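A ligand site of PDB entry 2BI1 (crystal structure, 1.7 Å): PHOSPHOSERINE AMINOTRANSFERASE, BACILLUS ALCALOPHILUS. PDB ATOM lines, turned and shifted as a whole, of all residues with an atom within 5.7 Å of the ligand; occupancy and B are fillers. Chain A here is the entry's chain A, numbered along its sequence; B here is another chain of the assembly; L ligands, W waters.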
ATOM      1  N   GLY A  74      17.817 -17.893   9.148  1.00  0.00           N
ATOM      2  CA  GLY A  74      18.479 -17.939  10.453  1.00  0.00           C
ATOM      3  C   GLY A  74      19.765 -17.137  10.482  1.00  0.00           C
ATOM      4  O   GLY A  74      20.320 -16.931  11.570  1.00  0.00           O
ATOM      5  N   GLY A  75      20.221 -16.703   9.314  1.00  0.00           N
ATOM      6  CA  GLY A  75      21.433 -15.882   9.308  1.00  0.00           C
ATOM      7  C   GLY A  75      22.695 -16.733   9.474  1.00  0.00           C
ATOM      8  O   GLY A  75      22.655 -17.944   9.708  1.00  0.00           O
ATOM      9  N   ALA A  76      23.836 -16.043   9.340  1.00  0.00           N
ATOM     10  CA  ALA A  76      25.103 -16.765   9.543  1.00  0.00           C
ATOM     11  C   ALA A  76      25.166 -17.277  10.964  1.00  0.00           C
ATOM     12  O   ALA A  76      25.742 -18.322  11.295  1.00  0.00           O
ATOM     13  CB  ALA A  76      26.265 -15.820   9.229  1.00  0.00           C
ATOM     14  N   SER A  77      24.555 -16.492  11.849  1.00  0.00           N
ATOM     15  CA  SER A  77      24.572 -16.851  13.266  1.00  0.00           C
ATOM     16  C   SER A  77      23.991 -18.229  13.496  1.00  0.00           C
ATOM     17  O   SER A  77      24.541 -18.972  14.321  1.00  0.00           O
ATOM     18  CB  SER A  77      23.840 -15.820  14.128  1.00  0.00           C
ATOM     19  OG  SER A  77      24.599 -14.625  14.121  1.00  0.00           O
ATOM     20  N   LEU A  78      22.922 -18.594  12.798  1.00  0.00           N
ATOM     21  CA  LEU A  78      22.396 -19.937  12.989  1.00  0.00           C
ATOM     22  C   LEU A  78      23.395 -20.985  12.466  1.00  0.00           C
ATOM     23  O   LEU A  78      23.464 -22.086  13.003  1.00  0.00           O
ATOM     24  CB  LEU A  78      21.043 -20.145  12.292  1.00  0.00           C
ATOM     25  CG  LEU A  78      20.373 -21.494  12.598  1.00  0.00           C
ATOM     26  CD1 LEU A  78      20.231 -21.666  14.100  1.00  0.00           C
ATOM     27  CD2 LEU A  78      19.025 -21.609  11.905  1.00  0.00           C
ATOM     28  N   PHE A  80      26.524 -20.866  12.783  1.00  0.00           N
ATOM     29  CA  PHE A  80      27.519 -21.089  13.839  1.00  0.00           C
ATOM     30  C   PHE A  80      27.176 -22.307  14.690  1.00  0.00           C
ATOM     31  O   PHE A  80      28.070 -23.019  15.157  1.00  0.00           O
ATOM     32  CB  PHE A  80      27.619 -19.876  14.753  1.00  0.00           C
ATOM     33  CG  PHE A  80      28.175 -18.594  14.157  1.00  0.00           C
ATOM     34  CD1 PHE A  80      27.963 -17.402  14.836  1.00  0.00           C
ATOM     35  CD2 PHE A  80      28.856 -18.591  12.948  1.00  0.00           C
ATOM     36  CE1 PHE A  80      28.450 -16.183  14.345  1.00  0.00           C
ATOM     37  CE2 PHE A  80      29.356 -17.402  12.474  1.00  0.00           C
ATOM     38  CZ  PHE A  80      29.165 -16.203  13.155  1.00  0.00           C
ATOM     39  N   TRP A 102      33.661 -12.116  14.679  1.00  0.00           N
ATOM     40  CA  TRP A 102      32.810 -13.161  14.110  1.00  0.00           C
ATOM     41  C   TRP A 102      33.458 -14.540  14.247  1.00  0.00           C
ATOM     42  O   TRP A 102      32.750 -15.528  14.509  1.00  0.00           O
ATOM     43  CB  TRP A 102      32.428 -12.884  12.647  1.00  0.00           C
ATOM     44  CG  TRP A 102      31.514 -11.681  12.577  1.00  0.00           C
ATOM     45  CD1 TRP A 102      31.758 -10.473  11.992  1.00  0.00           C
ATOM     46  CD2 TRP A 102      30.210 -11.602  13.128  1.00  0.00           C
ATOM     47  NE1 TRP A 102      30.687  -9.639  12.134  1.00  0.00           N
ATOM     48  CE2 TRP A 102      29.709 -10.309  12.832  1.00  0.00           C
ATOM     49  CE3 TRP A 102      29.398 -12.497  13.841  1.00  0.00           C
ATOM     50  CZ2 TRP A 102      28.446  -9.881  13.230  1.00  0.00           C
ATOM     51  CZ3 TRP A 102      28.150 -12.053  14.228  1.00  0.00           C
ATOM     52  CH2 TRP A 102      27.668 -10.774  13.927  1.00  0.00           C
ATOM     53  N   THR A 148      37.138 -17.454   8.990  1.00  0.00           N
ATOM     54  CA  THR A 148      36.318 -16.295   8.634  1.00  0.00           C
ATOM     55  C   THR A 148      37.052 -15.544   7.516  1.00  0.00           C
ATOM     56  O   THR A 148      38.050 -14.877   7.777  1.00  0.00           O
ATOM     57  CB  THR A 148      36.045 -15.417   9.847  1.00  0.00           C
ATOM     58  OG1 THR A 148      35.621 -16.264  10.924  1.00  0.00           O
ATOM     59  CG2 THR A 148      34.921 -14.416   9.560  1.00  0.00           C
ATOM     60  N   ASN A 150      36.498 -12.938   5.597  1.00  0.00           N
ATOM     61  CA  ASN A 150      36.533 -11.478   5.746  1.00  0.00           C
ATOM     62  C   ASN A 150      36.027 -11.092   7.143  1.00  0.00           C
ATOM     63  O   ASN A 150      34.885 -11.403   7.513  1.00  0.00           O
ATOM     64  CB  ASN A 150      35.703 -10.775   4.663  1.00  0.00           C
ATOM     65  CG  ASN A 150      35.879  -9.269   4.690  1.00  0.00           C
ATOM     66  OD1 ASN A 150      35.064  -8.521   5.234  1.00  0.00           O
ATOM     67  ND2 ASN A 150      36.972  -8.763   4.132  1.00  0.00           N
ATOM     68  N   ASN A 151      36.913 -10.443   7.916  1.00  0.00           N
ATOM     69  CA  ASN A 151      36.615 -10.110   9.301  1.00  0.00           C
ATOM     70  C   ASN A 151      35.975  -8.732   9.360  1.00  0.00           C
ATOM     71  O   ASN A 151      36.637  -7.708   9.454  1.00  0.00           O
ATOM     72  CB  ASN A 151      37.905 -10.220  10.120  1.00  0.00           C
ATOM     73  CG  ASN A 151      38.516 -11.591   9.881  1.00  0.00           C
ATOM     74  OD1 ASN A 151      38.050 -12.583  10.466  1.00  0.00           O
ATOM     75  ND2 ASN A 151      39.519 -11.681   9.043  1.00  0.00           N
ATOM     76  N   THR A 152      34.636  -8.781   9.272  1.00  0.00           N
ATOM     77  CA  THR A 152      33.826  -7.601   8.995  1.00  0.00           C
ATOM     78  C   THR A 152      34.086  -6.444   9.943  1.00  0.00           C
ATOM     79  O   THR A 152      34.001  -5.262   9.573  1.00  0.00           O
ATOM     80  CB  THR A 152      32.331  -7.995   9.075  1.00  0.00           C
ATOM     81  OG1 THR A 152      32.230  -9.334   8.585  1.00  0.00           O
ATOM     82  CG2 THR A 152      31.498  -7.120   8.164  1.00  0.00           C
ATOM     83  N   ASP A 172      33.106 -18.975   6.993  1.00  0.00           N
ATOM     84  CA  ASP A 172      32.113 -17.906   7.081  1.00  0.00           C
ATOM     85  C   ASP A 172      32.531 -16.805   6.099  1.00  0.00           C
ATOM     86  O   ASP A 172      33.440 -16.012   6.396  1.00  0.00           O
ATOM     87  CB  ASP A 172      32.035 -17.382   8.502  1.00  0.00           C
ATOM     88  CG  ASP A 172      31.092 -16.213   8.692  1.00  0.00           C
ATOM     89  OD1 ASP A 172      30.470 -15.785   7.690  1.00  0.00           O
ATOM     90  OD2 ASP A 172      30.988 -15.747   9.852  1.00  0.00           O
ATOM     91  N   MET A 173      31.860 -16.785   4.942  1.00  0.00           N
ATOM     92  CA  MET A 173      32.199 -15.743   3.950  1.00  0.00           C
ATOM     93  C   MET A 173      31.127 -14.659   3.849  1.00  0.00           C
ATOM     94  O   MET A 173      31.036 -14.063   2.788  1.00  0.00           O
ATOM     95  CB  MET A 173      32.399 -16.394   2.591  1.00  0.00           C
ATOM     96  CG  MET A 173      33.586 -17.369   2.543  1.00  0.00           C
ATOM     97  SD  MET A 173      33.957 -17.841   0.835  1.00  0.00           S
ATOM     98  CE  MET A 173      35.438 -18.844   1.081  1.00  0.00           C
ATOM     99  N   SER A 174      30.378 -14.417   4.910  1.00  0.00           N
ATOM    100  CA  SER A 174      29.277 -13.466   4.913  1.00  0.00           C
ATOM    101  C   SER A 174      29.636 -12.149   4.241  1.00  0.00           C
ATOM    102  O   SER A 174      28.888 -11.640   3.392  1.00  0.00           O
ATOM    103  CB  SER A 174      28.827 -13.198   6.350  1.00  0.00           C
ATOM    104  OG  SER A 174      28.285 -14.377   6.960  1.00  0.00           O
ATOM    105  N   SER A 175      30.821 -11.576   4.577  1.00  0.00           N
ATOM    106  CA  SER A 175      31.055 -10.218   4.075  1.00  0.00           C
ATOM    107  C   SER A 175      31.973 -10.146   2.866  1.00  0.00           C
ATOM    108  O   SER A 175      32.294  -9.000   2.488  1.00  0.00           O
ATOM    109  CB  SER A 175      31.562  -9.305   5.207  1.00  0.00           C
ATOM    110  OG  SER A 175      32.611  -9.933   5.926  1.00  0.00           O
ATOM    111  N   GLY A 193      25.451 -14.987   5.298  1.00  0.00           N
ATOM    112  CA  GLY A 193      24.170 -14.259   5.308  1.00  0.00           C
ATOM    113  C   GLY A 193      24.176 -13.429   4.021  1.00  0.00           C
ATOM    114  O   GLY A 193      25.166 -12.828   3.605  1.00  0.00           O
ATOM    115  N   GLN A 195      22.834 -10.553   3.347  1.00  0.00           N
ATOM    116  CA  GLN A 195      22.637  -9.118   3.509  1.00  0.00           C
ATOM    117  C   GLN A 195      23.929  -8.311   3.446  1.00  0.00           C
ATOM    118  O   GLN A 195      23.892  -7.092   3.549  1.00  0.00           O
ATOM    119  CB  GLN A 195      21.951  -8.772   4.837  1.00  0.00           C
ATOM    120  CG  GLN A 195      22.798  -9.081   6.074  1.00  0.00           C
ATOM    121  CD  GLN A 195      22.650 -10.511   6.550  1.00  0.00           C
ATOM    122  OE1 GLN A 195      22.203 -11.417   5.847  1.00  0.00           O
ATOM    123  NE2 GLN A 195      23.066 -10.748   7.794  1.00  0.00           N
ATOM    124  N   LYS A 196      25.082  -8.979   3.284  1.00  0.00           N
ATOM    125  CA  LYS A 196      26.234  -8.071   3.172  1.00  0.00           C
ATOM    126  C   LYS A 196      26.584  -7.827   1.726  1.00  0.00           C
ATOM    127  O   LYS A 196      26.755  -6.712   1.240  1.00  0.00           O
ATOM    128  CB  LYS A 196      27.419  -8.609   3.965  1.00  0.00           C
ATOM    129  CG  LYS A 196      27.090  -9.080   5.375  1.00  0.00           C
ATOM    130  CD  LYS A 196      27.663  -8.099   6.369  1.00  0.00           C
ATOM    131  CE  LYS A 196      27.010  -8.206   7.736  1.00  0.00           C
ATOM    132  NZ  LYS A 196      27.697  -9.217   8.590  1.00  0.00           N
ATOM    133  N   THR A 204      20.240 -17.101   3.987  1.00  0.00           N
ATOM    134  CA  THR A 204      21.641 -17.436   4.187  1.00  0.00           C
ATOM    135  C   THR A 204      22.051 -18.450   3.122  1.00  0.00           C
ATOM    136  O   THR A 204      21.383 -19.478   2.996  1.00  0.00           O
ATOM    137  CB  THR A 204      21.847 -18.028   5.602  1.00  0.00           C
ATOM    138  OG1 THR A 204      21.557 -16.986   6.535  1.00  0.00           O
ATOM    139  CG2 THR A 204      23.285 -18.453   5.804  1.00  0.00           C
ATOM    140  N   TYR A 338      31.143  -3.090  -0.091  1.00  0.00           N
ATOM    141  CA  TYR A 338      30.703  -4.301  -0.756  1.00  0.00           C
ATOM    142  C   TYR A 338      30.459  -4.097  -2.257  1.00  0.00           C
ATOM    143  O   TYR A 338      30.462  -2.941  -2.682  1.00  0.00           O
ATOM    144  CB  TYR A 338      29.386  -4.771  -0.113  1.00  0.00           C
ATOM    145  CG  TYR A 338      29.503  -5.016   1.368  1.00  0.00           C
ATOM    146  CD1 TYR A 338      28.737  -4.280   2.272  1.00  0.00           C
ATOM    147  CD2 TYR A 338      30.372  -5.975   1.869  1.00  0.00           C
ATOM    148  CE1 TYR A 338      28.828  -4.498   3.631  1.00  0.00           C
ATOM    149  CE2 TYR A 338      30.472  -6.195   3.230  1.00  0.00           C
ATOM    150  CZ  TYR A 338      29.709  -5.463   4.113  1.00  0.00           C
ATOM    151  OH  TYR A 338      29.791  -5.656   5.487  1.00  0.00           O
ATOM    152  N   HIS B  41      20.255  -2.831  10.355  1.00  0.00           N
ATOM    153  CA  HIS B  41      19.242  -3.158  11.342  1.00  0.00           C
ATOM    154  C   HIS B  41      19.519  -2.460  12.657  1.00  0.00           C
ATOM    155  O   HIS B  41      18.726  -2.487  13.598  1.00  0.00           O
ATOM    156  CB  HIS B  41      19.176  -4.679  11.550  1.00  0.00           C
ATOM    157  CG  HIS B  41      20.442  -5.280  12.048  1.00  0.00           C
ATOM    158  ND1 HIS B  41      21.634  -5.234  11.375  1.00  0.00           N
ATOM    159  CD2 HIS B  41      20.690  -5.941  13.216  1.00  0.00           C
ATOM    160  CE1 HIS B  41      22.566  -5.843  12.075  1.00  0.00           C
ATOM    161  NE2 HIS B  41      22.012  -6.296  13.203  1.00  0.00           N
ATOM    162  N   GLN B  73      13.444 -15.989  12.588  1.00  0.00           N
ATOM    163  CA  GLN B  73      13.510 -16.683  11.311  1.00  0.00           C
ATOM    164  C   GLN B  73      13.292 -18.183  11.534  1.00  0.00           C
ATOM    165  O   GLN B  73      13.331 -18.608  12.699  1.00  0.00           O
ATOM    166  CB  GLN B  73      14.882 -16.463  10.651  1.00  0.00           C
ATOM    167  CG  GLN B  73      15.207 -14.993  10.377  1.00  0.00           C
ATOM    168  CD  GLN B  73      16.571 -14.871   9.673  1.00  0.00           C
ATOM    169  OE1 GLN B  73      16.715 -15.359   8.553  1.00  0.00           O
ATOM    170  NE2 GLN B  73      17.526 -14.258  10.370  1.00  0.00           N
ATOM    171  N   ASN B 237      20.796 -10.995  16.163  1.00  0.00           N
ATOM    172  CA  ASN B 237      21.489 -11.019  14.857  1.00  0.00           C
ATOM    173  C   ASN B 237      20.610 -10.261  13.870  1.00  0.00           C
ATOM    174  O   ASN B 237      19.643  -9.603  14.256  1.00  0.00           O
ATOM    175  CB  ASN B 237      21.836 -12.405  14.347  1.00  0.00           C
ATOM    176  CG  ASN B 237      20.687 -13.236  13.860  1.00  0.00           C
ATOM    177  OD1 ASN B 237      19.569 -13.104  14.386  1.00  0.00           O
ATOM    178  ND2 ASN B 237      20.940 -14.065  12.861  1.00  0.00           N
ATOM    179  N   THR B 238      20.964 -10.297  12.611  1.00  0.00           N
ATOM    180  CA  THR B 238      20.259  -9.478  11.627  1.00  0.00           C
ATOM    181  C   THR B 238      18.865 -10.063  11.417  1.00  0.00           C
ATOM    182  O   THR B 238      18.766 -11.221  11.027  1.00  0.00           O
ATOM    183  CB  THR B 238      21.018  -9.448  10.290  1.00  0.00           C
ATOM    184  OG1 THR B 238      22.399  -9.091  10.479  1.00  0.00           O
ATOM    185  CG2 THR B 238      20.412  -8.380   9.375  1.00  0.00           C
HETATM  186  N1  LIG L   1      29.564 -13.528  10.175  1.00  0.00           N
HETATM  187  C1  LIG L   1      30.085 -12.467   9.513  1.00  0.00           C
HETATM  188  C2  LIG L   1      31.527 -12.495   8.993  1.00  0.00           C
HETATM  189  C3  LIG L   1      29.351 -11.334   9.349  1.00  0.00           C
HETATM  190  O1  LIG L   1      29.946 -10.280   8.729  1.00  0.00           O
HETATM  191  C4  LIG L   1      28.068 -11.297   9.859  1.00  0.00           C
HETATM  192  C5  LIG L   1      27.095 -10.130   9.500  1.00  0.00           C
HETATM  193  C6  LIG L   1      27.569 -12.342  10.583  1.00  0.00           C
HETATM  194  C7  LIG L   1      28.314 -13.478  10.739  1.00  0.00           C
HETATM  195  C8  LIG L   1      26.158 -12.273  11.203  1.00  0.00           C
HETATM  196  O2  LIG L   1      25.176 -12.684  10.258  1.00  0.00           O
HETATM  197  P1  LIG L   1      23.646 -12.763  10.715  1.00  0.00           P
HETATM  198  O3  LIG L   1      23.374 -11.448  11.321  1.00  0.00           O
HETATM  199  O4  LIG L   1      23.636 -13.891  11.688  1.00  0.00           O
HETATM  200  O5  LIG L   1      22.896 -13.047   9.491  1.00  0.00           O
HETATM  201  O   HOH W   1      25.842 -12.998   7.463  1.00  0.00           O
HETATM  202  O   HOH W   2      24.302 -10.174  13.574  1.00  0.00           O
HETATM  203  O   HOH W   3      26.166  -7.571  11.031  1.00  0.00           O
HETATM  204  O   HOH W   4      20.201 -12.976   9.580  1.00  0.00           O
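An oxygen (O5) of the ligand sits at hydrogen-bond distance from the side-chain amide nitrogen (NE2) of Gln 195 (2.9 Å). A nitrogen (N1) of the ligand lies within hydrogen-bond range of the side-chain carboxylate (OD2) of Asp 172 (2.7 Å). O5 of the ligand lies within hydrogen-bond range of N of Ala 76, at 3.1 Å. N of Thr 238 of chain B lies within hydrogen-bond range of O3 of the ligand. An oxygen (O4) of the ligand sits at hydrogen-bond distance from the side-chain amide nitrogen (ND2) of Asn 237 of chain B (2.9 Å). The side-chain amino group (NZ) of Lys 196 is bonded to a carbon (C5) of the ligand, at 1.4 Å. N of Ser 77 is in hydrogen-bond range of O4 of the ligand (2.8 Å). OG of Ser 77 is in hydrogen-bond range of O4 of the ligand (2.7 Å). O1 of the ligand is in hydrogen-bond range of OG1 of Thr 152. An oxygen (O3) of the ligand sits at hydrogen-bond distance from the side-chain hydroxyl (OG1) of Thr 238 of chain B (2.7 Å).
The side-chain amide oxygen (OD1) of Asn 150 is in hydrogen-bond range of the side-chain hydroxyl (OG) of Ser 175. OG1 of Thr 238 of chain B is in hydrogen-bond range of NE2 of Gln 195 (3.2 Å). The backbone carbonyl oxygen (O) of Gly 74 sits at hydrogen-bond distance from the side-chain amide nitrogen (ND2) of Asn 237 of chain B (3.2 Å). The side-chain hydroxyl (OG1) of Thr 152 lies within hydrogen-bond range of the side-chain hydroxyl (OG) of Ser 175 (2.8 Å). The side-chain carboxylate of Asp 172 lies within hydrogen-bond range of the side-chain hydroxyl of Ser 174, at 2.7 Å. The side-chain hydroxyl (OG) of Ser 174 sits at hydrogen-bond distance from the backbone NH (N) of Gly 193. O of Thr 238 of chain B is in hydrogen-bond range of NE2 of Gln 73 of chain B, at 3.3 Å. The backbone NH (N) of Gly 75 lies close to the side-chain hydroxyl (OG1) of Thr 204 (3.1 Å).
Gly 75 touches the ligand. CZ of Phe 80 touches C7 of the ligand, 3.7 Å away. Trp 102 touches the ligand. Thr 148 touches the ligand. Asn 150 touches the ligand (O to C2, 3.8 Å). Ser 174 touches the ligand (CB to C1, 3.5 Å). Ser 175 touches the ligand. Of the 24 residues printed, 15 come within 4 Å of the ligand.
Water W4 lies within hydrogen-bond range of the backbone carbonyl oxygen (O) of Thr 238 of chain B (2.7 Å), an oxygen (O5) of the ligand (2.7 Å) and the side-chain amide nitrogen (NE2) of Gln 73 of chain B (3.1 Å). Water W2 bridges an oxygen (O3) of the ligand (2.7 Å) and the backbone NH (N) of Thr 238 of chain B (3.5 Å). Water W1 lies within hydrogen-bond range of the side-chain hydroxyl of Ser 174 (2.9 Å), an oxygen (O2) of the ligand (2.9 Å) and the backbone NH of Gly 193 (3.0 Å).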
